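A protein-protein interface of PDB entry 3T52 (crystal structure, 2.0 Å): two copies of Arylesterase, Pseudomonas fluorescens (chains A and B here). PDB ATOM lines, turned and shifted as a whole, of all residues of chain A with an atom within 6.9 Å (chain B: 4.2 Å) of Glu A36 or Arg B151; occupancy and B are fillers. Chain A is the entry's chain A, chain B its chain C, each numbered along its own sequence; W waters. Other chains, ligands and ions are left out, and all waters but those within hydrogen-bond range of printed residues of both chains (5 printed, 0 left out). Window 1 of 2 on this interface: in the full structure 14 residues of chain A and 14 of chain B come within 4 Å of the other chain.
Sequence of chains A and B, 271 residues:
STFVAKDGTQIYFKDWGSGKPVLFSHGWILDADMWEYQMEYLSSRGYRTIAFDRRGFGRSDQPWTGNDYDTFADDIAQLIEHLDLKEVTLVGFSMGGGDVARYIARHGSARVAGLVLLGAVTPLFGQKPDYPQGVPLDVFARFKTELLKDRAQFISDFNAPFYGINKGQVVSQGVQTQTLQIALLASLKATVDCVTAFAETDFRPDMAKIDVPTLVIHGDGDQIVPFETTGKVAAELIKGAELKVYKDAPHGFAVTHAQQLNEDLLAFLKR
The side-chain carboxylate (OE1) of Glu A36 lies within salt-bridge range of the guanidinium group (NH1) of Arg B151 (2.7 Å). The backbone NH (N) of Arg B151 sits at hydrogen-bond distance from the side-chain hydroxyl (OH) of Tyr A37 (2.7 Å). The side-chain amide oxygen (OE1) of Gln B153 lies within hydrogen-bond range of the backbone NH (N) of Gly A174 (2.8 Å). NH1 of Arg B151 lies close to NE2 of Gln A178, at 3.3 Å.
The side-chain amide nitrogen (NE2) of Gln A178 is in hydrogen-bond range of the side-chain carboxylate (OE2) of Glu A36 (3.5 Å). OD1 of Asp B150 lies close to N of Ala B152. OD1 of Asp B150 is in hydrogen-bond range of N of Gln B153 (3.0 Å). The backbone carbonyl oxygen (O) of Ala B183 sits at hydrogen-bond distance from the guanidinium group (NH2) of Arg B151. O of Ala B186 lies within hydrogen-bond range of NH2 of Arg B151 (2.9 Å).
Among the printed residues, pairs that only touch across the chains: Gly A174 with Ala B152 (3.4 Å), Tyr A37 with Leu B147 (3.4 Å), Tyr A37 with Asp B150 (3.4 Å), Tyr A37 with Leu B188 (3.5 Å), Glu A36 with Leu B188 (3.6 Å), Val A175 with Asp B150 (3.6 Å), Val A175 with Ala B152 (3.8 Å), Gln A178 with Leu B184 (3.9 Å) and Gln A178 with Ala B152 (3.9 Å).
Glu A36 touches two residues of chain B. Of chain A, only Glu A36 (2.7 Å), Tyr A37 (2.7 Å) and Gln A178 (3.3 Å) come within 4 Å of Arg B151. Printed residues of chain B within 4 Å of Gln A178: Arg B151 (3.3 Å), Ala B152 (3.9 Å) and Leu B184 (3.9 Å). Printed residues of chain B within 4 Å of Val A175: Asp B150 and Ala B152. Of the printed residues of chain A, Leu B184 touches Gln A178 (3.9 Å). Printed residues of chain A within 4 Å of Ala B152: Gly A174 (3.4 Å), Val A175 (3.8 Å) and Gln A178 (3.9 Å). Tyr A41 touches none of the printed residues of chain B.
Of the 17 printed residues of chain A, 5 touch a printed residue of chain B. Hydrophobic or aromatic side chains of chain A that line the printed part of chain B: Tyr A37 and Val A175. Of the 11 printed residues of chain B, 7 touch a printed residue of chain A. Printed residues of chain B that touch a printed residue of chain A: Leu B147, Asp B150, Arg B151, Ala B152, Gln B153, Leu B184 and Leu B188.
No position is printed for both chains.
Water W2 lies within hydrogen-bond range of the side-chain carboxylate (OE1) of Glu A36 (2.5 Å), the backbone NH (N) of Leu B188 (3.0 Å) and the side-chain amino group (NZ) of Lys A14 (3.2 Å). Water W1 lies within hydrogen-bond range of O of Leu B184, OD2 of Asp A33 and NE2 of Gln A178. Water W3 lies within hydrogen-bond range of OH of Tyr A37, OD1 of Asp B150, N of Ala B152 and N of Arg B151. Water W4 lies within hydrogen-bond range of the backbone carbonyl oxygen (O) of Ala B186 (2.9 Å), the side-chain carboxylate (OD2) of Asp A33 (2.9 Å) and the side-chain amino group (NZ) of Lys A14 (3.4 Å). Water W5 bridges the side-chain amide oxygen (OE1) of Gln B153 (3.2 Å) and the backbone NH (N) of Gly A174 (3.3 Å).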
ATOM      1  N   LYS A  14      24.118  16.894  11.011  1.00  0.00           N
ATOM      2  CA  LYS A  14      23.096  17.884  11.318  1.00  0.00           C
ATOM      3  C   LYS A  14      22.862  17.841  12.824  1.00  0.00           C
ATOM      4  O   LYS A  14      22.863  16.779  13.414  1.00  0.00           O
ATOM      5  CB  LYS A  14      21.768  17.549  10.629  1.00  0.00           C
ATOM      6  CG  LYS A  14      21.912  17.224   9.153  1.00  0.00           C
ATOM      7  CD  LYS A  14      20.523  17.121   8.517  1.00  0.00           C
ATOM      8  CE  LYS A  14      20.625  16.552   7.100  1.00  0.00           C
ATOM      9  NZ  LYS A  14      19.257  16.506   6.451  1.00  0.00           N
ATOM     10  N   TRP A  16      20.042  19.440  15.311  1.00  0.00           N
ATOM     11  CA  TRP A  16      18.776  20.176  15.297  1.00  0.00           C
ATOM     12  C   TRP A  16      18.131  20.260  16.694  1.00  0.00           C
ATOM     13  O   TRP A  16      18.123  19.283  17.431  1.00  0.00           O
ATOM     14  CB  TRP A  16      17.781  19.487  14.372  1.00  0.00           C
ATOM     15  CG  TRP A  16      18.024  19.631  12.886  1.00  0.00           C
ATOM     16  CD1 TRP A  16      19.001  20.362  12.258  1.00  0.00           C
ATOM     17  CD2 TRP A  16      17.252  19.032  11.866  1.00  0.00           C
ATOM     18  NE1 TRP A  16      18.875  20.246  10.893  1.00  0.00           N
ATOM     19  CE2 TRP A  16      17.806  19.436  10.624  1.00  0.00           C
ATOM     20  CE3 TRP A  16      16.132  18.186  11.875  1.00  0.00           C
ATOM     21  CZ2 TRP A  16      17.280  19.021   9.395  1.00  0.00           C
ATOM     22  CZ3 TRP A  16      15.602  17.756  10.644  1.00  0.00           C
ATOM     23  CH2 TRP A  16      16.183  18.182   9.418  1.00  0.00           C
ATOM     24  N   ALA A  32      22.584  10.683   6.484  1.00  0.00           N
ATOM     25  CA  ALA A  32      21.807  11.277   7.582  1.00  0.00           C
ATOM     26  C   ALA A  32      20.367  11.623   7.187  1.00  0.00           C
ATOM     27  O   ALA A  32      19.500  11.715   8.057  1.00  0.00           O
ATOM     28  CB  ALA A  32      22.503  12.546   8.098  1.00  0.00           C
ATOM     29  N   ASP A  33      20.110  11.809   5.892  1.00  0.00           N
ATOM     30  CA  ASP A  33      18.752  12.154   5.453  1.00  0.00           C
ATOM     31  C   ASP A  33      17.749  11.056   5.726  1.00  0.00           C
ATOM     32  O   ASP A  33      16.537  11.345   5.774  1.00  0.00           O
ATOM     33  CB  ASP A  33      18.675  12.533   3.962  1.00  0.00           C
ATOM     34  CG  ASP A  33      19.343  13.850   3.644  1.00  0.00           C
ATOM     35  OD1 ASP A  33      19.918  14.518   4.563  1.00  0.00           O
ATOM     36  OD2 ASP A  33      19.346  14.210   2.428  1.00  0.00           O
ATOM     37  N   MET A  34      18.204   9.805   5.885  1.00  0.00           N
ATOM     38  CA  MET A  34      17.252   8.721   6.171  1.00  0.00           C
ATOM     39  C   MET A  34      16.477   8.978   7.477  1.00  0.00           C
ATOM     40  O   MET A  34      15.430   8.385   7.678  1.00  0.00           O
ATOM     41  CB  MET A  34      17.919   7.342   6.263  1.00  0.00           C
ATOM     42  CG  MET A  34      18.753   7.106   7.566  1.00  0.00           C
ATOM     43  SD  MET A  34      18.908   5.339   7.956  1.00  0.00           S
ATOM     44  CE  MET A  34      17.263   5.006   8.683  1.00  0.00           C
ATOM     45  N   TRP A  35      17.034   9.818   8.358  1.00  0.00           N
ATOM     46  CA  TRP A  35      16.437  10.134   9.657  1.00  0.00           C
ATOM     47  C   TRP A  35      15.573  11.408   9.710  1.00  0.00           C
ATOM     48  O   TRP A  35      15.098  11.763  10.805  1.00  0.00           O
ATOM     49  CB  TRP A  35      17.534  10.322  10.677  1.00  0.00           C
ATOM     50  CG  TRP A  35      18.406   9.104  10.877  1.00  0.00           C
ATOM     51  CD1 TRP A  35      19.748   8.970  10.545  1.00  0.00           C
ATOM     52  CD2 TRP A  35      18.005   7.860  11.440  1.00  0.00           C
ATOM     53  NE1 TRP A  35      20.181   7.710  10.876  1.00  0.00           N
ATOM     54  CE2 TRP A  35      19.142   7.017  11.453  1.00  0.00           C
ATOM     55  CE3 TRP A  35      16.792   7.371  11.956  1.00  0.00           C
ATOM     56  CZ2 TRP A  35      19.108   5.718  11.984  1.00  0.00           C
ATOM     57  CZ3 TRP A  35      16.755   6.071  12.451  1.00  0.00           C
ATOM     58  CH2 TRP A  35      17.916   5.261  12.471  1.00  0.00           C
ATOM     59  N   GLU A  36      15.382  12.088   8.571  1.00  0.00           N
ATOM     60  CA  GLU A  36      14.808  13.445   8.582  1.00  0.00           C
ATOM     61  C   GLU A  36      13.422  13.480   9.240  1.00  0.00           C
ATOM     62  O   GLU A  36      13.131  14.407   9.980  1.00  0.00           O
ATOM     63  CB  GLU A  36      14.777  14.080   7.179  1.00  0.00           C
ATOM     64  CG  GLU A  36      13.851  13.340   6.141  1.00  0.00           C
ATOM     65  CD  GLU A  36      14.229  13.639   4.661  1.00  0.00           C
ATOM     66  OE1 GLU A  36      15.075  14.529   4.407  1.00  0.00           O
ATOM     67  OE2 GLU A  36      13.678  12.985   3.742  1.00  0.00           O
ATOM     68  N   TYR A  37      12.592  12.477   8.978  1.00  0.00           N
ATOM     69  CA  TYR A  37      11.247  12.436   9.590  1.00  0.00           C
ATOM     70  C   TYR A  37      11.309  12.175  11.108  1.00  0.00           C
ATOM     71  O   TYR A  37      10.544  12.775  11.852  1.00  0.00           O
ATOM     72  CB  TYR A  37      10.346  11.406   8.905  1.00  0.00           C
ATOM     73  CG  TYR A  37      10.094  11.749   7.438  1.00  0.00           C
ATOM     74  CD1 TYR A  37       9.095  12.671   7.080  1.00  0.00           C
ATOM     75  CD2 TYR A  37      10.845  11.153   6.414  1.00  0.00           C
ATOM     76  CE1 TYR A  37       8.876  13.015   5.750  1.00  0.00           C
ATOM     77  CE2 TYR A  37      10.632  11.492   5.066  1.00  0.00           C
ATOM     78  CZ  TYR A  37       9.635  12.431   4.752  1.00  0.00           C
ATOM     79  OH  TYR A  37       9.383  12.792   3.450  1.00  0.00           O
ATOM     80  N   GLN A  38      12.222  11.306  11.562  1.00  0.00           N
ATOM     81  CA  GLN A  38      12.392  11.070  13.009  1.00  0.00           C
ATOM     82  C   GLN A  38      12.954  12.284  13.720  1.00  0.00           C
ATOM     83  O   GLN A  38      12.499  12.627  14.831  1.00  0.00           O
ATOM     84  CB  GLN A  38      13.264   9.830  13.299  1.00  0.00           C
ATOM     85  CG  GLN A  38      12.549   8.523  13.027  1.00  0.00           C
ATOM     86  CD  GLN A  38      12.383   8.224  11.535  1.00  0.00           C
ATOM     87  OE1 GLN A  38      13.343   8.328  10.757  1.00  0.00           O
ATOM     88  NE2 GLN A  38      11.164   7.841  11.128  1.00  0.00           N
ATOM     89  N   MET A  39      13.916  12.952  13.076  1.00  0.00           N
ATOM     90  CA  MET A  39      14.491  14.182  13.607  1.00  0.00           C
ATOM     91  C   MET A  39      13.484  15.327  13.719  1.00  0.00           C
ATOM     92  O   MET A  39      13.450  16.014  14.736  1.00  0.00           O
ATOM     93  CB  MET A  39      15.705  14.634  12.776  1.00  0.00           C
ATOM     94  CG  MET A  39      16.871  13.602  12.862  1.00  0.00           C
ATOM     95  SD  MET A  39      18.236  14.146  11.830  1.00  0.00           S
ATOM     96  CE  MET A  39      18.805  15.583  12.742  1.00  0.00           C
ATOM     97  N   GLU A  40      12.687  15.539  12.678  1.00  0.00           N
ATOM     98  CA  GLU A  40      11.638  16.553  12.732  1.00  0.00           C
ATOM     99  C   GLU A  40      10.648  16.222  13.846  1.00  0.00           C
ATOM    100  O   GLU A  40      10.308  17.086  14.630  1.00  0.00           O
ATOM    101  CB  GLU A  40      10.899  16.678  11.402  1.00  0.00           C
ATOM    102  CG  GLU A  40       9.926  17.866  11.339  1.00  0.00           C
ATOM    103  CD  GLU A  40       8.554  17.577  11.991  1.00  0.00           C
ATOM    104  OE1 GLU A  40       7.841  18.544  12.349  1.00  0.00           O
ATOM    105  OE2 GLU A  40       8.187  16.397  12.143  1.00  0.00           O
ATOM    106  N   TYR A  41      10.209  14.972  13.907  1.00  0.00           N
ATOM    107  CA  TYR A  41       9.228  14.538  14.901  1.00  0.00           C
ATOM    108  C   TYR A  41       9.682  14.804  16.337  1.00  0.00           C
ATOM    109  O   TYR A  41       8.915  15.349  17.154  1.00  0.00           O
ATOM    110  CB  TYR A  41       8.971  13.055  14.707  1.00  0.00           C
ATOM    111  CG  TYR A  41       7.870  12.502  15.571  1.00  0.00           C
ATOM    112  CD1 TYR A  41       6.538  12.581  15.163  1.00  0.00           C
ATOM    113  CD2 TYR A  41       8.157  11.928  16.814  1.00  0.00           C
ATOM    114  CE1 TYR A  41       5.515  12.062  15.952  1.00  0.00           C
ATOM    115  CE2 TYR A  41       7.137  11.409  17.617  1.00  0.00           C
ATOM    116  CZ  TYR A  41       5.816  11.492  17.178  1.00  0.00           C
ATOM    117  OH  TYR A  41       4.809  10.973  17.963  1.00  0.00           O
ATOM    118  N   ALA A  51      22.440  13.763  13.538  1.00  0.00           N
ATOM    119  CA  ALA A  51      22.683  12.634  12.640  1.00  0.00           C
ATOM    120  C   ALA A  51      23.843  12.993  11.697  1.00  0.00           C
ATOM    121  O   ALA A  51      23.895  14.116  11.186  1.00  0.00           O
ATOM    122  CB  ALA A  51      21.406  12.262  11.854  1.00  0.00           C
ATOM    123  N   GLY A 174       9.185   8.300  -5.699  1.00  0.00           N
ATOM    124  CA  GLY A 174       9.996   9.406  -5.163  1.00  0.00           C
ATOM    125  C   GLY A 174      10.992   8.936  -4.111  1.00  0.00           C
ATOM    126  O   GLY A 174      12.162   9.289  -4.153  1.00  0.00           O
ATOM    127  N   VAL A 175      10.531   8.131  -3.154  1.00  0.00           N
ATOM    128  CA  VAL A 175      11.411   7.585  -2.145  1.00  0.00           C
ATOM    129  C   VAL A 175      12.489   6.700  -2.789  1.00  0.00           C
ATOM    130  O   VAL A 175      13.623   6.701  -2.361  1.00  0.00           O
ATOM    131  CB  VAL A 175      10.643   6.761  -1.098  1.00  0.00           C
ATOM    132  CG1 VAL A 175      11.616   5.948  -0.260  1.00  0.00           C
ATOM    133  CG2 VAL A 175       9.819   7.677  -0.204  1.00  0.00           C
ATOM    134  N   GLN A 178      15.034   9.013  -4.378  1.00  0.00           N
ATOM    135  CA  GLN A 178      15.841   9.681  -3.348  1.00  0.00           C
ATOM    136  C   GLN A 178      16.886   8.713  -2.771  1.00  0.00           C
ATOM    137  O   GLN A 178      18.010   9.109  -2.483  1.00  0.00           O
ATOM    138  CB  GLN A 178      14.943  10.210  -2.227  1.00  0.00           C
ATOM    139  CG  GLN A 178      15.732  10.917  -1.099  1.00  0.00           C
ATOM    140  CD  GLN A 178      14.854  11.420   0.039  1.00  0.00           C
ATOM    141  OE1 GLN A 178      13.763  10.916   0.251  1.00  0.00           O
ATOM    142  NE2 GLN A 178      15.327  12.424   0.762  1.00  0.00           N
ATOM    143  N   ILE A 182      20.945   9.442  -3.044  1.00  0.00           N
ATOM    144  CA  ILE A 182      21.811   9.475  -1.843  1.00  0.00           C
ATOM    145  C   ILE A 182      22.901   8.395  -1.887  1.00  0.00           C
ATOM    146  O   ILE A 182      24.096   8.663  -1.593  1.00  0.00           O
ATOM    147  CB  ILE A 182      20.949   9.359  -0.555  1.00  0.00           C
ATOM    148  CG1 ILE A 182      20.135  10.651  -0.339  1.00  0.00           C
ATOM    149  CG2 ILE A 182      21.830   9.077   0.708  1.00  0.00           C
ATOM    150  CD1 ILE A 182      18.978  10.469   0.705  1.00  0.00           C
ATOM    151  N   LEU B 147       3.900  16.577   3.021  1.00  0.00           N
ATOM    152  CA  LEU B 147       5.364  16.686   3.050  1.00  0.00           C
ATOM    153  C   LEU B 147       5.948  15.904   4.225  1.00  0.00           C
ATOM    154  O   LEU B 147       7.023  15.313   4.102  1.00  0.00           O
ATOM    155  CB  LEU B 147       5.797  18.150   3.167  1.00  0.00           C
ATOM    156  CG  LEU B 147       5.570  18.964   1.906  1.00  0.00           C
ATOM    157  CD1 LEU B 147       5.598  20.491   2.280  1.00  0.00           C
ATOM    158  CD2 LEU B 147       6.636  18.631   0.871  1.00  0.00           C
ATOM    159  N   ASP B 150       5.725  12.080   2.949  1.00  0.00           N
ATOM    160  CA  ASP B 150       6.573  11.698   1.828  1.00  0.00           C
ATOM    161  C   ASP B 150       6.882  12.906   0.955  1.00  0.00           C
ATOM    162  O   ASP B 150       6.197  13.157  -0.054  1.00  0.00           O
ATOM    163  CB  ASP B 150       5.872  10.597   1.010  1.00  0.00           C
ATOM    164  CG  ASP B 150       6.749  10.028  -0.104  1.00  0.00           C
ATOM    165  OD1 ASP B 150       7.799  10.631  -0.438  1.00  0.00           O
ATOM    166  OD2 ASP B 150       6.359   8.975  -0.674  1.00  0.00           O
ATOM    167  N   ARG B 151       7.937  13.631   1.306  1.00  0.00           N
ATOM    168  CA  ARG B 151       8.257  14.828   0.551  1.00  0.00           C
ATOM    169  C   ARG B 151       8.743  14.552  -0.863  1.00  0.00           C
ATOM    170  O   ARG B 151       8.479  15.348  -1.773  1.00  0.00           O
ATOM    171  CB  ARG B 151       9.222  15.741   1.306  1.00  0.00           C
ATOM    172  CG  ARG B 151      10.610  15.254   1.370  1.00  0.00           C
ATOM    173  CD  ARG B 151      11.559  16.390   1.745  1.00  0.00           C
ATOM    174  NE  ARG B 151      12.842  15.794   2.061  1.00  0.00           N
ATOM    175  CZ  ARG B 151      14.003  16.184   1.559  1.00  0.00           C
ATOM    176  NH1 ARG B 151      15.093  15.528   1.923  1.00  0.00           N
ATOM    177  NH2 ARG B 151      14.071  17.223   0.717  1.00  0.00           N
ATOM    178  N   ALA B 152       9.446  13.437  -1.051  1.00  0.00           N
ATOM    179  CA  ALA B 152       9.980  13.058  -2.366  1.00  0.00           C
ATOM    180  C   ALA B 152       8.880  12.869  -3.409  1.00  0.00           C
ATOM    181  O   ALA B 152       8.995  13.382  -4.530  1.00  0.00           O
ATOM    182  CB  ALA B 152      10.874  11.775  -2.268  1.00  0.00           C
ATOM    183  N   GLN B 153       7.812  12.160  -3.035  1.00  0.00           N
ATOM    184  CA  GLN B 153       6.661  12.012  -3.926  1.00  0.00           C
ATOM    185  C   GLN B 153       5.858  13.313  -4.064  1.00  0.00           C
ATOM    186  O   GLN B 153       5.390  13.651  -5.163  1.00  0.00           O
ATOM    187  CB  GLN B 153       5.737  10.867  -3.497  1.00  0.00           C
ATOM    188  CG  GLN B 153       4.811  10.393  -4.678  1.00  0.00           C
ATOM    189  CD  GLN B 153       5.587  10.055  -5.977  1.00  0.00           C
ATOM    190  OE1 GLN B 153       6.657   9.430  -5.950  1.00  0.00           O
ATOM    191  NE2 GLN B 153       5.017  10.443  -7.124  1.00  0.00           N
ATOM    192  N   PHE B 154       5.733  14.058  -2.969  1.00  0.00           N
ATOM    193  CA  PHE B 154       5.160  15.398  -3.069  1.00  0.00           C
ATOM    194  C   PHE B 154       5.858  16.223  -4.161  1.00  0.00           C
ATOM    195  O   PHE B 154       5.213  16.756  -5.047  1.00  0.00           O
ATOM    196  CB  PHE B 154       5.172  16.144  -1.739  1.00  0.00           C
ATOM    197  CG  PHE B 154       4.400  17.460  -1.777  1.00  0.00           C
ATOM    198  CD1 PHE B 154       3.072  17.514  -1.341  1.00  0.00           C
ATOM    199  CD2 PHE B 154       4.992  18.622  -2.272  1.00  0.00           C
ATOM    200  CE1 PHE B 154       2.338  18.723  -1.387  1.00  0.00           C
ATOM    201  CE2 PHE B 154       4.278  19.845  -2.322  1.00  0.00           C
ATOM    202  CZ  PHE B 154       2.960  19.898  -1.873  1.00  0.00           C
ATOM    203  N   ILE B 155       7.178  16.338  -4.088  1.00  0.00           N
ATOM    204  CA  ILE B 155       7.917  17.137  -5.069  1.00  0.00           C
ATOM    205  C   ILE B 155       7.700  16.588  -6.474  1.00  0.00           C
ATOM    206  O   ILE B 155       7.524  17.334  -7.447  1.00  0.00           O
ATOM    207  CB  ILE B 155       9.425  17.103  -4.784  1.00  0.00           C
ATOM    208  CG1 ILE B 155       9.722  17.791  -3.442  1.00  0.00           C
ATOM    209  CG2 ILE B 155      10.193  17.834  -5.917  1.00  0.00           C
ATOM    210  CD1 ILE B 155      10.986  17.205  -2.764  1.00  0.00           C
ATOM    211  N   ALA B 183      15.530  19.607  -5.435  1.00  0.00           N
ATOM    212  CA  ALA B 183      14.591  19.666  -4.307  1.00  0.00           C
ATOM    213  C   ALA B 183      14.976  18.690  -3.198  1.00  0.00           C
ATOM    214  O   ALA B 183      14.829  18.990  -2.011  1.00  0.00           O
ATOM    215  CB  ALA B 183      13.153  19.409  -4.796  1.00  0.00           C
ATOM    216  N   LEU B 184      15.500  17.513  -3.568  1.00  0.00           N
ATOM    217  CA  LEU B 184      15.871  16.516  -2.555  1.00  0.00           C
ATOM    218  C   LEU B 184      17.127  16.898  -1.756  1.00  0.00           C
ATOM    219  O   LEU B 184      17.375  16.343  -0.664  1.00  0.00           O
ATOM    220  CB  LEU B 184      16.062  15.119  -3.196  1.00  0.00           C
ATOM    221  CG  LEU B 184      14.754  14.537  -3.779  1.00  0.00           C
ATOM    222  CD1 LEU B 184      15.085  13.297  -4.581  1.00  0.00           C
ATOM    223  CD2 LEU B 184      13.773  14.231  -2.649  1.00  0.00           C
ATOM    224  N   ALA B 186      17.418  19.660  -0.279  1.00  0.00           N
ATOM    225  CA  ALA B 186      16.904  20.478   0.830  1.00  0.00           C
ATOM    226  C   ALA B 186      16.577  19.678   2.091  1.00  0.00           C
ATOM    227  O   ALA B 186      16.295  18.474   2.032  1.00  0.00           O
ATOM    228  CB  ALA B 186      15.636  21.226   0.387  1.00  0.00           C
ATOM    229  N   LEU B 188      14.113  18.607   5.043  1.00  0.00           N
ATOM    230  CA  LEU B 188      12.688  18.395   5.297  1.00  0.00           C
ATOM    231  C   LEU B 188      12.127  19.532   6.170  1.00  0.00           C
ATOM    232  O   LEU B 188      11.032  20.063   5.904  1.00  0.00           O
ATOM    233  CB  LEU B 188      12.460  17.043   5.997  1.00  0.00           C
ATOM    234  CG  LEU B 188      11.035  16.843   6.541  1.00  0.00           C
ATOM    235  CD1 LEU B 188      10.080  16.762   5.351  1.00  0.00           C
ATOM    236  CD2 LEU B 188      10.977  15.572   7.399  1.00  0.00           C
HETATM  237  O   HOH W   1      17.892  13.938   0.117  1.00  0.00           O
HETATM  238  O   HOH W   2      16.242  16.540   5.419  1.00  0.00           O
HETATM  239  O   HOH W   3      10.209  11.371   1.150  1.00  0.00           O
HETATM  240  O   HOH W   4      18.417  16.869   3.158  1.00  0.00           O
HETATM  241  O   HOH W   5       8.541  10.020  -8.467  1.00  0.00           O
